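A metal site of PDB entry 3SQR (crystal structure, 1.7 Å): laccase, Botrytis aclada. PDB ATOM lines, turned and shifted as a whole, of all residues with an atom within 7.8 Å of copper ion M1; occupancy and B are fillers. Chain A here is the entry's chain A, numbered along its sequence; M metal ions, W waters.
The side-chain hydroxyl (OH) of Tyr 175 lies within hydrogen-bond range of the backbone carbonyl oxygen (O) of His 527 (3.0 Å). OD1 of Asp 500 sits at hydrogen-bond distance from NE2 of His 126. The backbone NH of His 126 is in hydrogen-bond range of the backbone carbonyl oxygen of Trp 166, 2.9 Å away. O of Gly 308 is in hydrogen-bond range of NE2 of His 126, 3.4 Å away. A ring nitrogen (NE2) of His 126 lies within hydrogen-bond range of a ring nitrogen (NE2) of His 466. OG1 of Thr 165 is in hydrogen-bond range of O of His 126, 2.5 Å away. NE2 of His 126 sits close to NH1 of Arg 310, at 3.2 Å. The backbone NH of His 168 is in hydrogen-bond range of the backbone carbonyl oxygen of His 124 (2.9 Å).
Copper ion M1 is bound by ND1 of His 126, NE2 of His 168 and NE2 of His 527. Copper ion M1 has three donor atoms within binding distance. Slightly farther from copper ion M1 lies water W1 (2.6 Å).
Residues that only touch copper ion M1: Trp 166. Of the 23 residues printed, 4 come within 4 Å of copper ion M1. The nearest printed residue that does not touch copper ion M1 is His 466 (4.01 Å).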
ATOM      1  N   HIS A 124      -3.143 -15.890  23.855  1.00  0.00           N
ATOM      2  CA  HIS A 124      -2.911 -14.863  22.873  1.00  0.00           C
ATOM      3  C   HIS A 124      -4.038 -13.783  22.957  1.00  0.00           C
ATOM      4  O   HIS A 124      -5.180 -14.041  23.174  1.00  0.00           O
ATOM      5  CB  HIS A 124      -2.854 -15.470  21.477  1.00  0.00           C
ATOM      6  CG  HIS A 124      -2.862 -14.460  20.380  1.00  0.00           C
ATOM      7  ND1 HIS A 124      -1.814 -13.577  20.188  1.00  0.00           N
ATOM      8  CD2 HIS A 124      -3.733 -14.242  19.364  1.00  0.00           C
ATOM      9  CE1 HIS A 124      -2.109 -12.789  19.162  1.00  0.00           C
ATOM     10  NE2 HIS A 124      -3.244 -13.186  18.624  1.00  0.00           N
ATOM     11  N   TRP A 125      -3.601 -12.557  22.752  1.00  0.00           N
ATOM     12  CA  TRP A 125      -4.457 -11.351  22.859  1.00  0.00           C
ATOM     13  C   TRP A 125      -4.617 -10.928  21.408  1.00  0.00           C
ATOM     14  O   TRP A 125      -3.698 -10.376  20.779  1.00  0.00           O
ATOM     15  CB  TRP A 125      -3.760 -10.325  23.766  1.00  0.00           C
ATOM     16  CG  TRP A 125      -3.105 -11.011  24.923  1.00  0.00           C
ATOM     17  CD1 TRP A 125      -1.789 -11.460  24.997  1.00  0.00           C
ATOM     18  CD2 TRP A 125      -3.738 -11.467  26.113  1.00  0.00           C
ATOM     19  NE1 TRP A 125      -1.615 -12.138  26.151  1.00  0.00           N
ATOM     20  CE2 TRP A 125      -2.794 -12.205  26.834  1.00  0.00           C
ATOM     21  CE3 TRP A 125      -5.062 -11.404  26.606  1.00  0.00           C
ATOM     22  CZ2 TRP A 125      -3.090 -12.852  27.985  1.00  0.00           C
ATOM     23  CZ3 TRP A 125      -5.371 -12.058  27.773  1.00  0.00           C
ATOM     24  CH2 TRP A 125      -4.374 -12.766  28.481  1.00  0.00           C
ATOM     25  N   HIS A 126      -5.771 -11.316  20.824  1.00  0.00           N
ATOM     26  CA  HIS A 126      -5.900 -11.286  19.396  1.00  0.00           C
ATOM     27  C   HIS A 126      -5.816  -9.879  18.835  1.00  0.00           C
ATOM     28  O   HIS A 126      -6.572  -9.000  19.157  1.00  0.00           O
ATOM     29  CB  HIS A 126      -7.117 -12.096  18.923  1.00  0.00           C
ATOM     30  CG  HIS A 126      -7.186 -12.176  17.458  1.00  0.00           C
ATOM     31  ND1 HIS A 126      -7.206 -13.352  16.774  1.00  0.00           N
ATOM     32  CD2 HIS A 126      -7.321 -11.202  16.527  1.00  0.00           C
ATOM     33  CE1 HIS A 126      -7.310 -13.106  15.486  1.00  0.00           C
ATOM     34  NE2 HIS A 126      -7.342 -11.800  15.298  1.00  0.00           N
ATOM     35  N   GLY A 127      -4.922  -9.729  17.863  1.00  0.00           N
ATOM     36  CA  GLY A 127      -4.766  -8.497  17.147  1.00  0.00           C
ATOM     37  C   GLY A 127      -3.989  -7.443  17.913  1.00  0.00           C
ATOM     38  O   GLY A 127      -3.775  -6.346  17.396  1.00  0.00           O
ATOM     39  N   THR A 165     -11.788  -6.869  20.365  1.00  0.00           N
ATOM     40  CA  THR A 165     -11.065  -8.086  20.075  1.00  0.00           C
ATOM     41  C   THR A 165     -11.390  -9.121  21.123  1.00  0.00           C
ATOM     42  O   THR A 165     -12.401  -9.028  21.833  1.00  0.00           O
ATOM     43  CB  THR A 165      -9.551  -7.853  19.810  1.00  0.00           C
ATOM     44  OG1 THR A 165      -9.047  -9.028  19.171  1.00  0.00           O
ATOM     45  CG2 THR A 165      -8.771  -7.513  21.117  1.00  0.00           C
ATOM     46  N   TRP A 166     -10.530 -10.136  21.182  1.00  0.00           N
ATOM     47  CA  TRP A 166     -10.788 -11.271  22.018  1.00  0.00           C
ATOM     48  C   TRP A 166      -9.429 -11.819  22.412  1.00  0.00           C
ATOM     49  O   TRP A 166      -8.456 -11.510  21.777  1.00  0.00           O
ATOM     50  CB  TRP A 166     -11.640 -12.306  21.313  1.00  0.00           C
ATOM     51  CG  TRP A 166     -11.131 -12.894  20.001  1.00  0.00           C
ATOM     52  CD1 TRP A 166     -10.697 -12.212  18.875  1.00  0.00           C
ATOM     53  CD2 TRP A 166     -11.114 -14.283  19.647  1.00  0.00           C
ATOM     54  NE1 TRP A 166     -10.451 -13.115  17.853  1.00  0.00           N
ATOM     55  CE2 TRP A 166     -10.658 -14.375  18.311  1.00  0.00           C
ATOM     56  CE3 TRP A 166     -11.418 -15.451  20.327  1.00  0.00           C
ATOM     57  CZ2 TRP A 166     -10.457 -15.624  17.687  1.00  0.00           C
ATOM     58  CZ3 TRP A 166     -11.269 -16.676  19.712  1.00  0.00           C
ATOM     59  CH2 TRP A 166     -10.775 -16.771  18.393  1.00  0.00           C
ATOM     60  N   TYR A 167      -9.423 -12.593  23.475  1.00  0.00           N
ATOM     61  CA  TYR A 167      -8.194 -13.310  23.874  1.00  0.00           C
ATOM     62  C   TYR A 167      -8.539 -14.761  23.842  1.00  0.00           C
ATOM     63  O   TYR A 167      -9.685 -15.156  24.114  1.00  0.00           O
ATOM     64  CB  TYR A 167      -7.687 -12.867  25.240  1.00  0.00           C
ATOM     65  CG  TYR A 167      -8.623 -13.127  26.385  1.00  0.00           C
ATOM     66  CD1 TYR A 167      -9.674 -12.307  26.657  1.00  0.00           C
ATOM     67  CD2 TYR A 167      -8.409 -14.202  27.249  1.00  0.00           C
ATOM     68  CE1 TYR A 167     -10.536 -12.554  27.759  1.00  0.00           C
ATOM     69  CE2 TYR A 167      -9.238 -14.443  28.319  1.00  0.00           C
ATOM     70  CZ  TYR A 167     -10.321 -13.620  28.561  1.00  0.00           C
ATOM     71  OH  TYR A 167     -11.132 -13.910  29.595  1.00  0.00           O
ATOM     72  N   HIS A 168      -7.537 -15.613  23.562  1.00  0.00           N
ATOM     73  CA  HIS A 168      -7.860 -17.005  23.476  1.00  0.00           C
ATOM     74  C   HIS A 168      -6.628 -17.828  23.609  1.00  0.00           C
ATOM     75  O   HIS A 168      -5.559 -17.362  23.341  1.00  0.00           O
ATOM     76  CB  HIS A 168      -8.556 -17.364  22.173  1.00  0.00           C
ATOM     77  CG  HIS A 168      -7.801 -17.012  20.918  1.00  0.00           C
ATOM     78  ND1 HIS A 168      -6.855 -17.838  20.343  1.00  0.00           N
ATOM     79  CD2 HIS A 168      -7.937 -15.957  20.072  1.00  0.00           C
ATOM     80  CE1 HIS A 168      -6.413 -17.271  19.226  1.00  0.00           C
ATOM     81  NE2 HIS A 168      -7.082 -16.143  19.020  1.00  0.00           N
ATOM     82  N   SER A 169      -6.807 -19.061  23.982  1.00  0.00           N
ATOM     83  CA  SER A 169      -5.618 -19.933  23.945  1.00  0.00           C
ATOM     84  C   SER A 169      -5.112 -20.061  22.527  1.00  0.00           C
ATOM     85  O   SER A 169      -5.900 -20.157  21.589  1.00  0.00           O
ATOM     86  CB  SER A 169      -5.932 -21.320  24.484  1.00  0.00           C
ATOM     87  OG  SER A 169      -4.800 -22.164  24.253  1.00  0.00           O
ATOM     88  N   HIS A 170      -3.778 -20.051  22.380  1.00  0.00           N
ATOM     89  CA  HIS A 170      -3.191 -20.309  21.110  1.00  0.00           C
ATOM     90  C   HIS A 170      -2.410 -21.640  21.223  1.00  0.00           C
ATOM     91  O   HIS A 170      -1.605 -21.971  20.384  1.00  0.00           O
ATOM     92  CB  HIS A 170      -2.274 -19.178  20.713  1.00  0.00           C
ATOM     93  CG  HIS A 170      -2.278 -18.880  19.257  1.00  0.00           C
ATOM     94  ND1 HIS A 170      -1.967 -19.798  18.308  1.00  0.00           N
ATOM     95  CD2 HIS A 170      -2.597 -17.734  18.571  1.00  0.00           C
ATOM     96  CE1 HIS A 170      -2.027 -19.249  17.115  1.00  0.00           C
ATOM     97  NE2 HIS A 170      -2.436 -17.994  17.237  1.00  0.00           N
ATOM     98  N   TYR A 175      -9.051 -23.288  22.194  1.00  0.00           N
ATOM     99  CA  TYR A 175     -10.147 -22.287  22.152  1.00  0.00           C
ATOM    100  C   TYR A 175     -11.420 -22.884  21.589  1.00  0.00           C
ATOM    101  O   TYR A 175     -12.535 -22.334  21.800  1.00  0.00           O
ATOM    102  CB  TYR A 175      -9.749 -20.950  21.475  1.00  0.00           C
ATOM    103  CG  TYR A 175      -9.867 -20.908  19.961  1.00  0.00           C
ATOM    104  CD1 TYR A 175     -11.063 -20.686  19.376  1.00  0.00           C
ATOM    105  CD2 TYR A 175      -8.791 -21.125  19.151  1.00  0.00           C
ATOM    106  CE1 TYR A 175     -11.227 -20.631  18.044  1.00  0.00           C
ATOM    107  CE2 TYR A 175      -8.939 -21.082  17.732  1.00  0.00           C
ATOM    108  CZ  TYR A 175     -10.158 -20.820  17.211  1.00  0.00           C
ATOM    109  OH  TYR A 175     -10.411 -20.758  15.848  1.00  0.00           O
ATOM    110  N   ASN A 269     -16.340 -13.634  15.235  1.00  0.00           N
ATOM    111  CA  ASN A 269     -16.459 -15.039  14.858  1.00  0.00           C
ATOM    112  C   ASN A 269     -15.286 -15.797  15.522  1.00  0.00           C
ATOM    113  O   ASN A 269     -14.161 -15.569  15.211  1.00  0.00           O
ATOM    114  CB  ASN A 269     -16.467 -15.195  13.327  1.00  0.00           C
ATOM    115  CG  ASN A 269     -16.423 -16.626  12.841  1.00  0.00           C
ATOM    116  OD1 ASN A 269     -16.280 -17.636  13.586  1.00  0.00           O
ATOM    117  ND2 ASN A 269     -16.498 -16.738  11.471  1.00  0.00           N
ATOM    118  N   VAL A 270     -15.628 -16.690  16.405  1.00  0.00           N
ATOM    119  CA  VAL A 270     -14.651 -17.437  17.225  1.00  0.00           C
ATOM    120  C   VAL A 270     -14.820 -18.935  17.104  1.00  0.00           C
ATOM    121  O   VAL A 270     -14.356 -19.701  17.975  1.00  0.00           O
ATOM    122  CB  VAL A 270     -14.718 -17.004  18.717  1.00  0.00           C
ATOM    123  CG1 VAL A 270     -14.408 -15.507  18.823  1.00  0.00           C
ATOM    124  CG2 VAL A 270     -16.067 -17.408  19.380  1.00  0.00           C
ATOM    125  N   ILE A 307     -13.288 -16.286  10.587  1.00  0.00           N
ATOM    126  CA  ILE A 307     -12.857 -16.652  11.915  1.00  0.00           C
ATOM    127  C   ILE A 307     -11.777 -15.709  12.418  1.00  0.00           C
ATOM    128  O   ILE A 307     -10.784 -15.487  11.752  1.00  0.00           O
ATOM    129  CB  ILE A 307     -12.339 -18.081  12.034  1.00  0.00           C
ATOM    130  CG1 ILE A 307     -13.411 -19.091  11.607  1.00  0.00           C
ATOM    131  CG2 ILE A 307     -11.965 -18.349  13.540  1.00  0.00           C
ATOM    132  CD1 ILE A 307     -12.850 -20.477  11.462  1.00  0.00           C
ATOM    133  N   GLY A 308     -11.989 -15.163  13.570  1.00  0.00           N
ATOM    134  CA  GLY A 308     -11.041 -14.248  14.190  1.00  0.00           C
ATOM    135  C   GLY A 308     -11.237 -12.790  13.804  1.00  0.00           C
ATOM    136  O   GLY A 308     -10.693 -11.909  14.507  1.00  0.00           O
ATOM    137  N   GLN A 309     -12.058 -12.560  12.773  1.00  0.00           N
ATOM    138  CA  GLN A 309     -12.497 -11.230  12.416  1.00  0.00           C
ATOM    139  C   GLN A 309     -13.493 -10.648  13.419  1.00  0.00           C
ATOM    140  O   GLN A 309     -14.289 -11.399  14.029  1.00  0.00           O
ATOM    141  CB  GLN A 309     -13.110 -11.206  11.038  1.00  0.00           C
ATOM    142  CG  GLN A 309     -12.138 -11.413   9.974  1.00  0.00           C
ATOM    143  CD  GLN A 309     -12.694 -11.132   8.599  1.00  0.00           C
ATOM    144  OE1 GLN A 309     -13.852 -11.415   8.325  1.00  0.00           O
ATOM    145  NE2 GLN A 309     -11.833 -10.691   7.686  1.00  0.00           N
ATOM    146  N   ARG A 310     -13.448  -9.307  13.571  1.00  0.00           N
ATOM    147  CA  ARG A 310     -14.344  -8.544  14.379  1.00  0.00           C
ATOM    148  C   ARG A 310     -14.903  -7.508  13.500  1.00  0.00           C
ATOM    149  O   ARG A 310     -14.238  -7.078  12.584  1.00  0.00           O
ATOM    150  CB  ARG A 310     -13.693  -7.851  15.600  1.00  0.00           C
ATOM    151  CG  ARG A 310     -13.222  -8.834  16.640  1.00  0.00           C
ATOM    152  CD  ARG A 310     -11.903  -9.406  16.300  1.00  0.00           C
ATOM    153  NE  ARG A 310     -10.870  -8.421  16.444  1.00  0.00           N
ATOM    154  CZ  ARG A 310      -9.678  -8.432  15.829  1.00  0.00           C
ATOM    155  NH1 ARG A 310      -9.389  -9.343  14.926  1.00  0.00           N
ATOM    156  NH2 ARG A 310      -8.799  -7.488  16.111  1.00  0.00           N
ATOM    157  N   HIS A 466      -4.600 -14.837   9.803  1.00  0.00           N
ATOM    158  CA  HIS A 466      -4.320 -13.937  10.895  1.00  0.00           C
ATOM    159  C   HIS A 466      -2.816 -13.701  10.945  1.00  0.00           C
ATOM    160  O   HIS A 466      -2.044 -14.671  10.955  1.00  0.00           O
ATOM    161  CB  HIS A 466      -4.757 -14.594  12.200  1.00  0.00           C
ATOM    162  CG  HIS A 466      -4.382 -13.805  13.417  1.00  0.00           C
ATOM    163  ND1 HIS A 466      -4.058 -14.386  14.631  1.00  0.00           N
ATOM    164  CD2 HIS A 466      -4.370 -12.471  13.600  1.00  0.00           C
ATOM    165  CE1 HIS A 466      -3.770 -13.413  15.484  1.00  0.00           C
ATOM    166  NE2 HIS A 466      -3.961 -12.253  14.879  1.00  0.00           N
ATOM    167  N   HIS A 468       0.104 -11.954  13.366  1.00  0.00           N
ATOM    168  CA  HIS A 468       0.397 -11.454  14.691  1.00  0.00           C
ATOM    169  C   HIS A 468       1.342 -10.226  14.578  1.00  0.00           C
ATOM    170  O   HIS A 468       2.085 -10.075  13.601  1.00  0.00           O
ATOM    171  CB  HIS A 468       1.078 -12.572  15.485  1.00  0.00           C
ATOM    172  CG  HIS A 468       0.170 -13.660  15.905  1.00  0.00           C
ATOM    173  ND1 HIS A 468       0.054 -14.070  17.212  1.00  0.00           N
ATOM    174  CD2 HIS A 468      -0.672 -14.440  15.190  1.00  0.00           C
ATOM    175  CE1 HIS A 468      -0.859 -15.019  17.287  1.00  0.00           C
ATOM    176  NE2 HIS A 468      -1.298 -15.269  16.085  1.00  0.00           N
ATOM    177  N   ASP A 500      -6.413  -7.280  10.962  1.00  0.00           N
ATOM    178  CA  ASP A 500      -5.472  -8.383  11.307  1.00  0.00           C
ATOM    179  C   ASP A 500      -5.862  -9.804  10.956  1.00  0.00           C
ATOM    180  O   ASP A 500      -5.037 -10.710  11.026  1.00  0.00           O
ATOM    181  CB  ASP A 500      -5.099  -8.279  12.815  1.00  0.00           C
ATOM    182  CG  ASP A 500      -6.287  -8.430  13.743  1.00  0.00           C
ATOM    183  OD1 ASP A 500      -6.865  -9.534  13.726  1.00  0.00           O
ATOM    184  OD2 ASP A 500      -6.624  -7.429  14.455  1.00  0.00           O
ATOM    185  N   VAL A 501      -7.092  -9.974  10.451  1.00  0.00           N
ATOM    186  CA  VAL A 501      -7.522 -11.287   9.898  1.00  0.00           C
ATOM    187  C   VAL A 501      -8.185 -11.023   8.552  1.00  0.00           C
ATOM    188  O   VAL A 501      -9.075 -10.177   8.432  1.00  0.00           O
ATOM    189  CB  VAL A 501      -8.493 -12.064  10.801  1.00  0.00           C
ATOM    190  CG1 VAL A 501      -8.948 -13.316  10.112  1.00  0.00           C
ATOM    191  CG2 VAL A 501      -7.888 -12.415  12.122  1.00  0.00           C
ATOM    192  N   HIS A 525      -1.128 -17.435  10.218  1.00  0.00           N
ATOM    193  CA  HIS A 525      -1.743 -18.704  10.084  1.00  0.00           C
ATOM    194  C   HIS A 525      -3.191 -18.585   9.720  1.00  0.00           C
ATOM    195  O   HIS A 525      -3.797 -17.538   9.922  1.00  0.00           O
ATOM    196  CB  HIS A 525      -1.637 -19.483  11.377  1.00  0.00           C
ATOM    197  CG  HIS A 525      -2.381 -18.871  12.510  1.00  0.00           C
ATOM    198  ND1 HIS A 525      -3.594 -19.344  12.954  1.00  0.00           N
ATOM    199  CD2 HIS A 525      -2.091 -17.797  13.281  1.00  0.00           C
ATOM    200  CE1 HIS A 525      -3.985 -18.622  13.989  1.00  0.00           C
ATOM    201  NE2 HIS A 525      -3.107 -17.651  14.180  1.00  0.00           N
ATOM    202  N   HIS A 527      -6.830 -19.295  10.661  1.00  0.00           N
ATOM    203  CA  HIS A 527      -7.477 -19.304  11.957  1.00  0.00           C
ATOM    204  C   HIS A 527      -8.548 -20.387  12.058  1.00  0.00           C
ATOM    205  O   HIS A 527      -9.212 -20.522  13.125  1.00  0.00           O
ATOM    206  CB  HIS A 527      -8.124 -17.914  12.274  1.00  0.00           C
ATOM    207  CG  HIS A 527      -7.984 -17.491  13.709  1.00  0.00           C
ATOM    208  ND1 HIS A 527      -8.517 -18.224  14.732  1.00  0.00           N
ATOM    209  CD2 HIS A 527      -7.399 -16.389  14.288  1.00  0.00           C
ATOM    210  CE1 HIS A 527      -8.262 -17.619  15.879  1.00  0.00           C
ATOM    211  NE2 HIS A 527      -7.564 -16.511  15.646  1.00  0.00           N
HETATM  212 CU    CU M   1      -6.989 -15.267  17.226  1.00  0.00          CU
HETATM  213 CU    CU M   2      -2.803 -16.552  15.813  1.00  0.00          CU
HETATM  214  O   HOH W   1      -4.724 -16.485  16.631  1.00  0.00           O
